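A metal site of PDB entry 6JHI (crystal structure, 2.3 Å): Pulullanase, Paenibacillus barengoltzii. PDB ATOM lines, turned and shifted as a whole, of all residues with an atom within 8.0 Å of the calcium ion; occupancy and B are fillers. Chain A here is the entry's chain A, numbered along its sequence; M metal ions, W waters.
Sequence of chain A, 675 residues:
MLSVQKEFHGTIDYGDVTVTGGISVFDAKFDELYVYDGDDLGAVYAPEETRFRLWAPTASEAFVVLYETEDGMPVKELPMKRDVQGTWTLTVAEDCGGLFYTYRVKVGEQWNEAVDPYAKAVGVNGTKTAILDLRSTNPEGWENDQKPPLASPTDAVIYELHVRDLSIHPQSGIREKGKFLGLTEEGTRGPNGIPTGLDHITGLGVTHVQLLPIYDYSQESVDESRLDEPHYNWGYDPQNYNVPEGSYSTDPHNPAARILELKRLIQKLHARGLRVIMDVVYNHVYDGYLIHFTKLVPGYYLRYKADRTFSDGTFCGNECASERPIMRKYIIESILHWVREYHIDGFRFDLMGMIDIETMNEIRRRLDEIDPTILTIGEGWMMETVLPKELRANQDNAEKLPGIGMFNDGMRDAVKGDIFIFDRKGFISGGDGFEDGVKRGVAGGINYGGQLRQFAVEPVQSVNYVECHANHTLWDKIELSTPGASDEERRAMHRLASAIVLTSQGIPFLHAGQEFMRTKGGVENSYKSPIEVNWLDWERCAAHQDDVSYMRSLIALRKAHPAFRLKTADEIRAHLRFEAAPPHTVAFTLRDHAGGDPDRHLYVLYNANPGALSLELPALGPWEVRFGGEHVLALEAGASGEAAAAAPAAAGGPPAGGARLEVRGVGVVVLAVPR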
ATOM      1  N   VAL A 122      24.273  -1.387 -13.437  1.00  0.00           N
ATOM      2  CA  VAL A 122      25.638  -1.893 -13.319  1.00  0.00           C
ATOM      3  C   VAL A 122      26.223  -2.051 -14.711  1.00  0.00           C
ATOM      4  O   VAL A 122      25.509  -2.090 -15.707  1.00  0.00           O
ATOM      5  CB  VAL A 122      25.699  -3.258 -12.593  1.00  0.00           C
ATOM      6  CG1 VAL A 122      25.204  -3.127 -11.158  1.00  0.00           C
ATOM      7  CG2 VAL A 122      24.903  -4.328 -13.388  1.00  0.00           C
ATOM      8  N   GLY A 123      27.550  -2.166 -14.771  1.00  0.00           N
ATOM      9  CA  GLY A 123      28.213  -2.539 -15.999  1.00  0.00           C
ATOM     10  C   GLY A 123      28.096  -4.033 -16.250  1.00  0.00           C
ATOM     11  O   GLY A 123      27.433  -4.776 -15.528  1.00  0.00           O
ATOM     12  N   VAL A 124      28.764  -4.478 -17.323  1.00  0.00           N
ATOM     13  CA  VAL A 124      28.755  -5.903 -17.652  1.00  0.00           C
ATOM     14  C   VAL A 124      29.289  -6.713 -16.472  1.00  0.00           C
ATOM     15  O   VAL A 124      30.228  -6.306 -15.768  1.00  0.00           O
ATOM     16  CB  VAL A 124      29.565  -6.159 -18.932  1.00  0.00           C
ATOM     17  CG1 VAL A 124      31.064  -5.905 -18.690  1.00  0.00           C
ATOM     18  CG2 VAL A 124      29.306  -7.578 -19.452  1.00  0.00           C
ATOM     19  N   ASN A 125      28.661  -7.859 -16.220  1.00  0.00           N
ATOM     20  CA  ASN A 125      28.982  -8.767 -15.132  1.00  0.00           C
ATOM     21  C   ASN A 125      28.878  -8.122 -13.748  1.00  0.00           C
ATOM     22  O   ASN A 125      29.299  -8.728 -12.752  1.00  0.00           O
ATOM     23  CB  ASN A 125      30.370  -9.404 -15.327  1.00  0.00           C
ATOM     24  CG  ASN A 125      30.318 -10.588 -16.291  1.00  0.00           C
ATOM     25  OD1 ASN A 125      29.297 -11.275 -16.380  1.00  0.00           O
ATOM     26  ND2 ASN A 125      31.408 -10.818 -17.018  1.00  0.00           N
ATOM     27  N   GLY A 126      28.343  -6.911 -13.668  1.00  0.00           N
ATOM     28  CA  GLY A 126      27.927  -6.325 -12.401  1.00  0.00           C
ATOM     29  C   GLY A 126      29.008  -6.017 -11.395  1.00  0.00           C
ATOM     30  O   GLY A 126      28.732  -6.061 -10.184  1.00  0.00           O
ATOM     31  N   TYR A 215      16.698 -10.925 -11.394  1.00  0.00           N
ATOM     32  CA  TYR A 215      17.727 -10.110 -10.757  1.00  0.00           C
ATOM     33  C   TYR A 215      19.092 -10.542 -11.314  1.00  0.00           C
ATOM     34  O   TYR A 215      19.218 -11.573 -11.976  1.00  0.00           O
ATOM     35  CB  TYR A 215      17.662 -10.271  -9.221  1.00  0.00           C
ATOM     36  CG  TYR A 215      17.833 -11.725  -8.790  1.00  0.00           C
ATOM     37  CD1 TYR A 215      19.098 -12.326  -8.761  1.00  0.00           C
ATOM     38  CD2 TYR A 215      16.731 -12.522  -8.474  1.00  0.00           C
ATOM     39  CE1 TYR A 215      19.270 -13.652  -8.403  1.00  0.00           C
ATOM     40  CE2 TYR A 215      16.889 -13.868  -8.116  1.00  0.00           C
ATOM     41  CZ  TYR A 215      18.169 -14.420  -8.096  1.00  0.00           C
ATOM     42  OH  TYR A 215      18.389 -15.734  -7.761  1.00  0.00           O
ATOM     43  N   ASP A 216      20.115  -9.756 -11.012  1.00  0.00           N
ATOM     44  CA  ASP A 216      21.442 -10.028 -11.565  1.00  0.00           C
ATOM     45  C   ASP A 216      22.113 -11.158 -10.795  1.00  0.00           C
ATOM     46  O   ASP A 216      22.418 -11.005  -9.604  1.00  0.00           O
ATOM     47  CB  ASP A 216      22.276  -8.754 -11.535  1.00  0.00           C
ATOM     48  CG  ASP A 216      23.618  -8.919 -12.214  1.00  0.00           C
ATOM     49  OD1 ASP A 216      23.712  -9.741 -13.139  1.00  0.00           O
ATOM     50  OD2 ASP A 216      24.576  -8.234 -11.812  1.00  0.00           O
ATOM     51  N   TYR A 217      22.363 -12.292 -11.447  1.00  0.00           N
ATOM     52  CA  TYR A 217      23.028 -13.404 -10.791  1.00  0.00           C
ATOM     53  C   TYR A 217      24.494 -13.508 -11.229  1.00  0.00           C
ATOM     54  O   TYR A 217      24.970 -12.777 -12.100  1.00  0.00           O
ATOM     55  CB  TYR A 217      22.262 -14.726 -11.002  1.00  0.00           C
ATOM     56  CG  TYR A 217      21.828 -15.123 -12.409  1.00  0.00           C
ATOM     57  CD1 TYR A 217      22.708 -15.790 -13.262  1.00  0.00           C
ATOM     58  CD2 TYR A 217      20.512 -14.919 -12.861  1.00  0.00           C
ATOM     59  CE1 TYR A 217      22.331 -16.189 -14.520  1.00  0.00           C
ATOM     60  CE2 TYR A 217      20.113 -15.315 -14.130  1.00  0.00           C
ATOM     61  CZ  TYR A 217      21.040 -15.954 -14.954  1.00  0.00           C
ATOM     62  OH  TYR A 217      20.697 -16.387 -16.201  1.00  0.00           O
ATOM     63  N   SER A 218      25.244 -14.400 -10.572  1.00  0.00           N
ATOM     64  CA  SER A 218      26.698 -14.325 -10.618  1.00  0.00           C
ATOM     65  C   SER A 218      27.269 -14.667 -11.998  1.00  0.00           C
ATOM     66  O   SER A 218      26.684 -15.425 -12.780  1.00  0.00           O
ATOM     67  CB  SER A 218      27.345 -15.253  -9.591  1.00  0.00           C
ATOM     68  OG  SER A 218      27.193 -16.606  -9.969  1.00  0.00           O
ATOM     69  N   GLN A 219      28.428 -14.071 -12.278  1.00  0.00           N
ATOM     70  CA  GLN A 219      29.180 -14.376 -13.488  1.00  0.00           C
ATOM     71  C   GLN A 219      29.557 -15.850 -13.563  1.00  0.00           C
ATOM     72  O   GLN A 219      29.685 -16.406 -14.648  1.00  0.00           O
ATOM     73  CB  GLN A 219      30.416 -13.490 -13.526  1.00  0.00           C
ATOM     74  CG  GLN A 219      31.494 -13.868 -14.511  1.00  0.00           C
ATOM     75  CD  GLN A 219      32.493 -12.732 -14.692  1.00  0.00           C
ATOM     76  OE1 GLN A 219      32.569 -11.804 -13.877  1.00  0.00           O
ATOM     77  NE2 GLN A 219      33.254 -12.786 -15.784  1.00  0.00           N
ATOM     78  N   GLU A 220      29.749 -16.496 -12.401  1.00  0.00           N
ATOM     79  CA  GLU A 220      30.021 -17.938 -12.374  1.00  0.00           C
ATOM     80  C   GLU A 220      28.889 -18.751 -13.011  1.00  0.00           C
ATOM     81  O   GLU A 220      29.137 -19.834 -13.551  1.00  0.00           O
ATOM     82  CB  GLU A 220      30.245 -18.375 -10.923  1.00  0.00           C
ATOM     83  CG  GLU A 220      30.137 -19.872 -10.665  1.00  0.00           C
ATOM     84  CD  GLU A 220      31.307 -20.660 -11.253  1.00  0.00           C
ATOM     85  OE1 GLU A 220      32.331 -20.032 -11.623  1.00  0.00           O
ATOM     86  OE2 GLU A 220      31.206 -21.907 -11.333  1.00  0.00           O
ATOM     87  N   SER A 221      27.654 -18.249 -12.961  1.00  0.00           N
ATOM     88  CA  SER A 221      26.525 -18.966 -13.530  1.00  0.00           C
ATOM     89  C   SER A 221      26.418 -18.721 -15.035  1.00  0.00           C
ATOM     90  O   SER A 221      26.365 -19.670 -15.824  1.00  0.00           O
ATOM     91  CB  SER A 221      25.227 -18.549 -12.840  1.00  0.00           C
ATOM     92  OG  SER A 221      25.352 -18.588 -11.426  1.00  0.00           O
ATOM     93  N   VAL A 222      26.347 -17.445 -15.427  1.00  0.00           N
ATOM     94  CA  VAL A 222      26.375 -17.040 -16.831  1.00  0.00           C
ATOM     95  C   VAL A 222      27.314 -15.843 -16.947  1.00  0.00           C
ATOM     96  O   VAL A 222      27.118 -14.824 -16.264  1.00  0.00           O
ATOM     97  CB  VAL A 222      24.977 -16.683 -17.388  1.00  0.00           C
ATOM     98  CG1 VAL A 222      25.079 -16.205 -18.838  1.00  0.00           C
ATOM     99  CG2 VAL A 222      24.039 -17.876 -17.314  1.00  0.00           C
ATOM    100  N   ASP A 223      28.327 -15.973 -17.790  1.00  0.00           N
ATOM    101  CA  ASP A 223      29.295 -14.905 -18.029  1.00  0.00           C
ATOM    102  C   ASP A 223      28.724 -13.965 -19.098  1.00  0.00           C
ATOM    103  O   ASP A 223      28.657 -14.329 -20.271  1.00  0.00           O
ATOM    104  CB  ASP A 223      30.636 -15.498 -18.464  1.00  0.00           C
ATOM    105  CG  ASP A 223      31.729 -14.441 -18.616  1.00  0.00           C
ATOM    106  OD1 ASP A 223      31.438 -13.230 -18.796  1.00  0.00           O
ATOM    107  OD2 ASP A 223      32.915 -14.845 -18.582  1.00  0.00           O
ATOM    108  N   GLU A 224      28.352 -12.744 -18.685  1.00  0.00           N
ATOM    109  CA  GLU A 224      27.725 -11.789 -19.598  1.00  0.00           C
ATOM    110  C   GLU A 224      28.646 -11.314 -20.714  1.00  0.00           C
ATOM    111  O   GLU A 224      28.162 -10.675 -21.669  1.00  0.00           O
ATOM    112  CB  GLU A 224      27.206 -10.583 -18.809  1.00  0.00           C
ATOM    113  CG  GLU A 224      26.118 -10.945 -17.791  1.00  0.00           C
ATOM    114  CD  GLU A 224      25.681  -9.740 -16.972  1.00  0.00           C
ATOM    115  OE1 GLU A 224      26.018  -8.605 -17.372  1.00  0.00           O
ATOM    116  OE2 GLU A 224      24.997  -9.928 -15.928  1.00  0.00           O
ATOM    117  N   ASP A 237      21.806 -17.598  -7.764  1.00  0.00           N
ATOM    118  CA  ASP A 237      23.109 -17.222  -7.223  1.00  0.00           C
ATOM    119  C   ASP A 237      23.186 -15.708  -7.233  1.00  0.00           C
ATOM    120  O   ASP A 237      23.806 -15.105  -8.125  1.00  0.00           O
ATOM    121  CB  ASP A 237      24.253 -17.832  -8.053  1.00  0.00           C
ATOM    122  CG  ASP A 237      24.085 -19.325  -8.254  1.00  0.00           C
ATOM    123  OD1 ASP A 237      24.052 -20.056  -7.234  1.00  0.00           O
ATOM    124  OD2 ASP A 237      23.999 -19.775  -9.425  1.00  0.00           O
ATOM    125  N   GLN A 239      23.819 -11.803  -7.047  1.00  0.00           N
ATOM    126  CA  GLN A 239      24.918 -10.848  -6.936  1.00  0.00           C
ATOM    127  C   GLN A 239      24.445  -9.411  -6.722  1.00  0.00           C
ATOM    128  O   GLN A 239      24.924  -8.747  -5.796  1.00  0.00           O
ATOM    129  CB  GLN A 239      25.822 -10.930  -8.180  1.00  0.00           C
ATOM    130  CG  GLN A 239      27.141 -10.203  -8.005  1.00  0.00           C
ATOM    131  CD  GLN A 239      27.996 -10.248  -9.260  1.00  0.00           C
ATOM    132  OE1 GLN A 239      28.096 -11.291  -9.931  1.00  0.00           O
ATOM    133  NE2 GLN A 239      28.623  -9.122  -9.587  1.00  0.00           N
ATOM    134  N   ASN A 240      23.541  -8.894  -7.548  1.00  0.00           N
ATOM    135  CA  ASN A 240      23.005  -7.538  -7.345  1.00  0.00           C
ATOM    136  C   ASN A 240      21.484  -7.612  -7.306  1.00  0.00           C
ATOM    137  O   ASN A 240      20.835  -7.794  -8.338  1.00  0.00           O
ATOM    138  CB  ASN A 240      23.461  -6.567  -8.417  1.00  0.00           C
ATOM    139  CG  ASN A 240      24.969  -6.351  -8.403  1.00  0.00           C
ATOM    140  OD1 ASN A 240      25.542  -5.963  -7.383  1.00  0.00           O
ATOM    141  ND2 ASN A 240      25.610  -6.619  -9.530  1.00  0.00           N
ATOM    142  N   VAL A 243      19.085  -4.949  -9.642  1.00  0.00           N
ATOM    143  CA  VAL A 243      19.360  -4.722 -11.069  1.00  0.00           C
ATOM    144  C   VAL A 243      18.923  -5.948 -11.874  1.00  0.00           C
ATOM    145  O   VAL A 243      19.086  -7.079 -11.404  1.00  0.00           O
ATOM    146  CB  VAL A 243      20.856  -4.470 -11.316  1.00  0.00           C
ATOM    147  CG1 VAL A 243      21.100  -3.986 -12.759  1.00  0.00           C
ATOM    148  CG2 VAL A 243      21.404  -3.477 -10.318  1.00  0.00           C
ATOM    149  N   PRO A 244      18.412  -5.786 -13.108  1.00  0.00           N
ATOM    150  CA  PRO A 244      18.102  -6.960 -13.919  1.00  0.00           C
ATOM    151  C   PRO A 244      19.354  -7.719 -14.341  1.00  0.00           C
ATOM    152  O   PRO A 244      20.463  -7.187 -14.380  1.00  0.00           O
ATOM    153  CB  PRO A 244      17.375  -6.359 -15.129  1.00  0.00           C
ATOM    154  CG  PRO A 244      16.796  -5.076 -14.622  1.00  0.00           C
ATOM    155  CD  PRO A 244      17.873  -4.563 -13.709  1.00  0.00           C
ATOM    156  N   GLU A 245      19.137  -9.002 -14.683  1.00  0.00           N
ATOM    157  CA  GLU A 245      20.205  -9.864 -15.173  1.00  0.00           C
ATOM    158  C   GLU A 245      20.676  -9.445 -16.554  1.00  0.00           C
ATOM    159  O   GLU A 245      19.857  -9.190 -17.458  1.00  0.00           O
ATOM    160  CB  GLU A 245      19.741 -11.327 -15.205  1.00  0.00           C
ATOM    161  CG  GLU A 245      20.516 -12.249 -16.154  1.00  0.00           C
ATOM    162  CD  GLU A 245      21.967 -12.465 -15.749  1.00  0.00           C
ATOM    163  OE1 GLU A 245      22.327 -12.158 -14.591  1.00  0.00           O
ATOM    164  OE2 GLU A 245      22.764 -12.952 -16.593  1.00  0.00           O
ATOM    165  N   GLY A 246      22.001  -9.411 -16.745  1.00  0.00           N
ATOM    166  CA  GLY A 246      22.559  -8.853 -17.952  1.00  0.00           C
ATOM    167  C   GLY A 246      22.383  -9.721 -19.183  1.00  0.00           C
ATOM    168  O   GLY A 246      22.170  -9.218 -20.292  1.00  0.00           O
ATOM    169  N   SER A 247      22.474 -11.047 -19.001  1.00  0.00           N
ATOM    170  CA  SER A 247      22.412 -11.943 -20.154  1.00  0.00           C
ATOM    171  C   SER A 247      21.039 -11.940 -20.827  1.00  0.00           C
ATOM    172  O   SER A 247      20.912 -12.431 -21.955  1.00  0.00           O
ATOM    173  CB  SER A 247      22.798 -13.370 -19.752  1.00  0.00           C
ATOM    174  OG  SER A 247      21.751 -14.054 -19.090  1.00  0.00           O
ATOM    175  N   TYR A 248      20.010 -11.416 -20.168  1.00  0.00           N
ATOM    176  CA  TYR A 248      18.687 -11.337 -20.745  1.00  0.00           C
ATOM    177  C   TYR A 248      18.436 -10.030 -21.508  1.00  0.00           C
ATOM    178  O   TYR A 248      17.338  -9.833 -22.027  1.00  0.00           O
ATOM    179  CB  TYR A 248      17.616 -11.532 -19.659  1.00  0.00           C
ATOM    180  CG  TYR A 248      17.689 -12.862 -18.915  1.00  0.00           C
ATOM    181  CD1 TYR A 248      18.195 -14.012 -19.525  1.00  0.00           C
ATOM    182  CD2 TYR A 248      17.243 -12.962 -17.594  1.00  0.00           C
ATOM    183  CE1 TYR A 248      18.258 -15.226 -18.840  1.00  0.00           C
ATOM    184  CE2 TYR A 248      17.300 -14.172 -16.896  1.00  0.00           C
ATOM    185  CZ  TYR A 248      17.812 -15.302 -17.518  1.00  0.00           C
ATOM    186  OH  TYR A 248      17.868 -16.492 -16.811  1.00  0.00           O
ATOM    187  N   PRO A 252      24.416  -6.381 -22.725  1.00  0.00           N
ATOM    188  CA  PRO A 252      24.775  -6.313 -21.302  1.00  0.00           C
ATOM    189  C   PRO A 252      25.783  -5.225 -20.983  1.00  0.00           C
ATOM    190  O   PRO A 252      25.961  -4.882 -19.808  1.00  0.00           O
ATOM    191  CB  PRO A 252      25.345  -7.709 -21.020  1.00  0.00           C
ATOM    192  CG  PRO A 252      25.764  -8.233 -22.379  1.00  0.00           C
ATOM    193  CD  PRO A 252      24.824  -7.648 -23.366  1.00  0.00           C
ATOM    194  N   ARG A 258      19.156  -3.453 -20.241  1.00  0.00           N
ATOM    195  CA  ARG A 258      18.436  -4.478 -19.478  1.00  0.00           C
ATOM    196  C   ARG A 258      17.255  -3.883 -18.726  1.00  0.00           C
ATOM    197  O   ARG A 258      16.214  -4.536 -18.591  1.00  0.00           O
ATOM    198  CB  ARG A 258      19.403  -5.185 -18.512  1.00  0.00           C
ATOM    199  CG  ARG A 258      20.025  -4.272 -17.454  1.00  0.00           C
ATOM    200  CD  ARG A 258      20.983  -5.043 -16.585  1.00  0.00           C
ATOM    201  NE  ARG A 258      22.285  -5.200 -17.221  1.00  0.00           N
ATOM    202  CZ  ARG A 258      23.297  -5.882 -16.681  1.00  0.00           C
ATOM    203  NH1 ARG A 258      23.150  -6.474 -15.499  1.00  0.00           N
ATOM    204  NH2 ARG A 258      24.469  -5.979 -17.315  1.00  0.00           N
HETATM  205 CA    CA M   1      24.790 -11.537 -14.060  1.00  0.00          CA
HETATM  206  O   HOH W   1      25.024 -13.718 -15.233  1.00  0.00           O
HETATM  207  O   HOH W   2      27.062 -11.496 -13.941  1.00  0.00           O
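The nearest printed residue that does not touch the calcium ion is Gly 246 (4.4 Å).
The backbone NH (N) of Gly 246 lies close to the side-chain carboxylate (OE2) of Glu 224. The side-chain hydroxyl (OH) of Tyr 217 sits at hydrogen-bond distance from the side-chain hydroxyl (OH) of Tyr 248. The side-chain carboxylate of Asp 216 sits at hydrogen-bond distance from the side-chain amide nitrogen of Asn 240 (3.0 Å). OD1 of Asn 125 sits at hydrogen-bond distance from N of Glu 224, at 2.9 Å. The backbone NH (N) of Gln 239 sits at hydrogen-bond distance from the backbone carbonyl oxygen (O) of Asp 216 (3.0 Å). The side-chain hydroxyl (OG) of Ser 247 sits at hydrogen-bond distance from the side-chain carboxylate (OE2) of Glu 245 (2.9 Å). The backbone NH (N) of Asp 216 lies within hydrogen-bond range of the backbone carbonyl oxygen (O) of Val 243. The guanidinium group (NH2) of Arg 258 is in salt-bridge range of the side-chain carboxylate (OE1) of Glu 224 (3.0 Å).
Water W2 lies within hydrogen-bond range of OD1 of Asn 125 (3.3 Å) and N of Gln 219 (3.4 Å).
Water W2 binds the calcium ion (2.3 Å). The calcium ion is bound by OD1 of Asp 216 (2.3 Å). The calcium ion is bound by O of Tyr 217, 2.3 Å away. The calcium ion is bound by the side-chain carboxylate (OE2) of Glu 224, at 2.5 Å. Water W1 is bound to the calcium ion (2.5 Å). OE1 of Glu 245 binds the calcium ion (2.6 Å).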
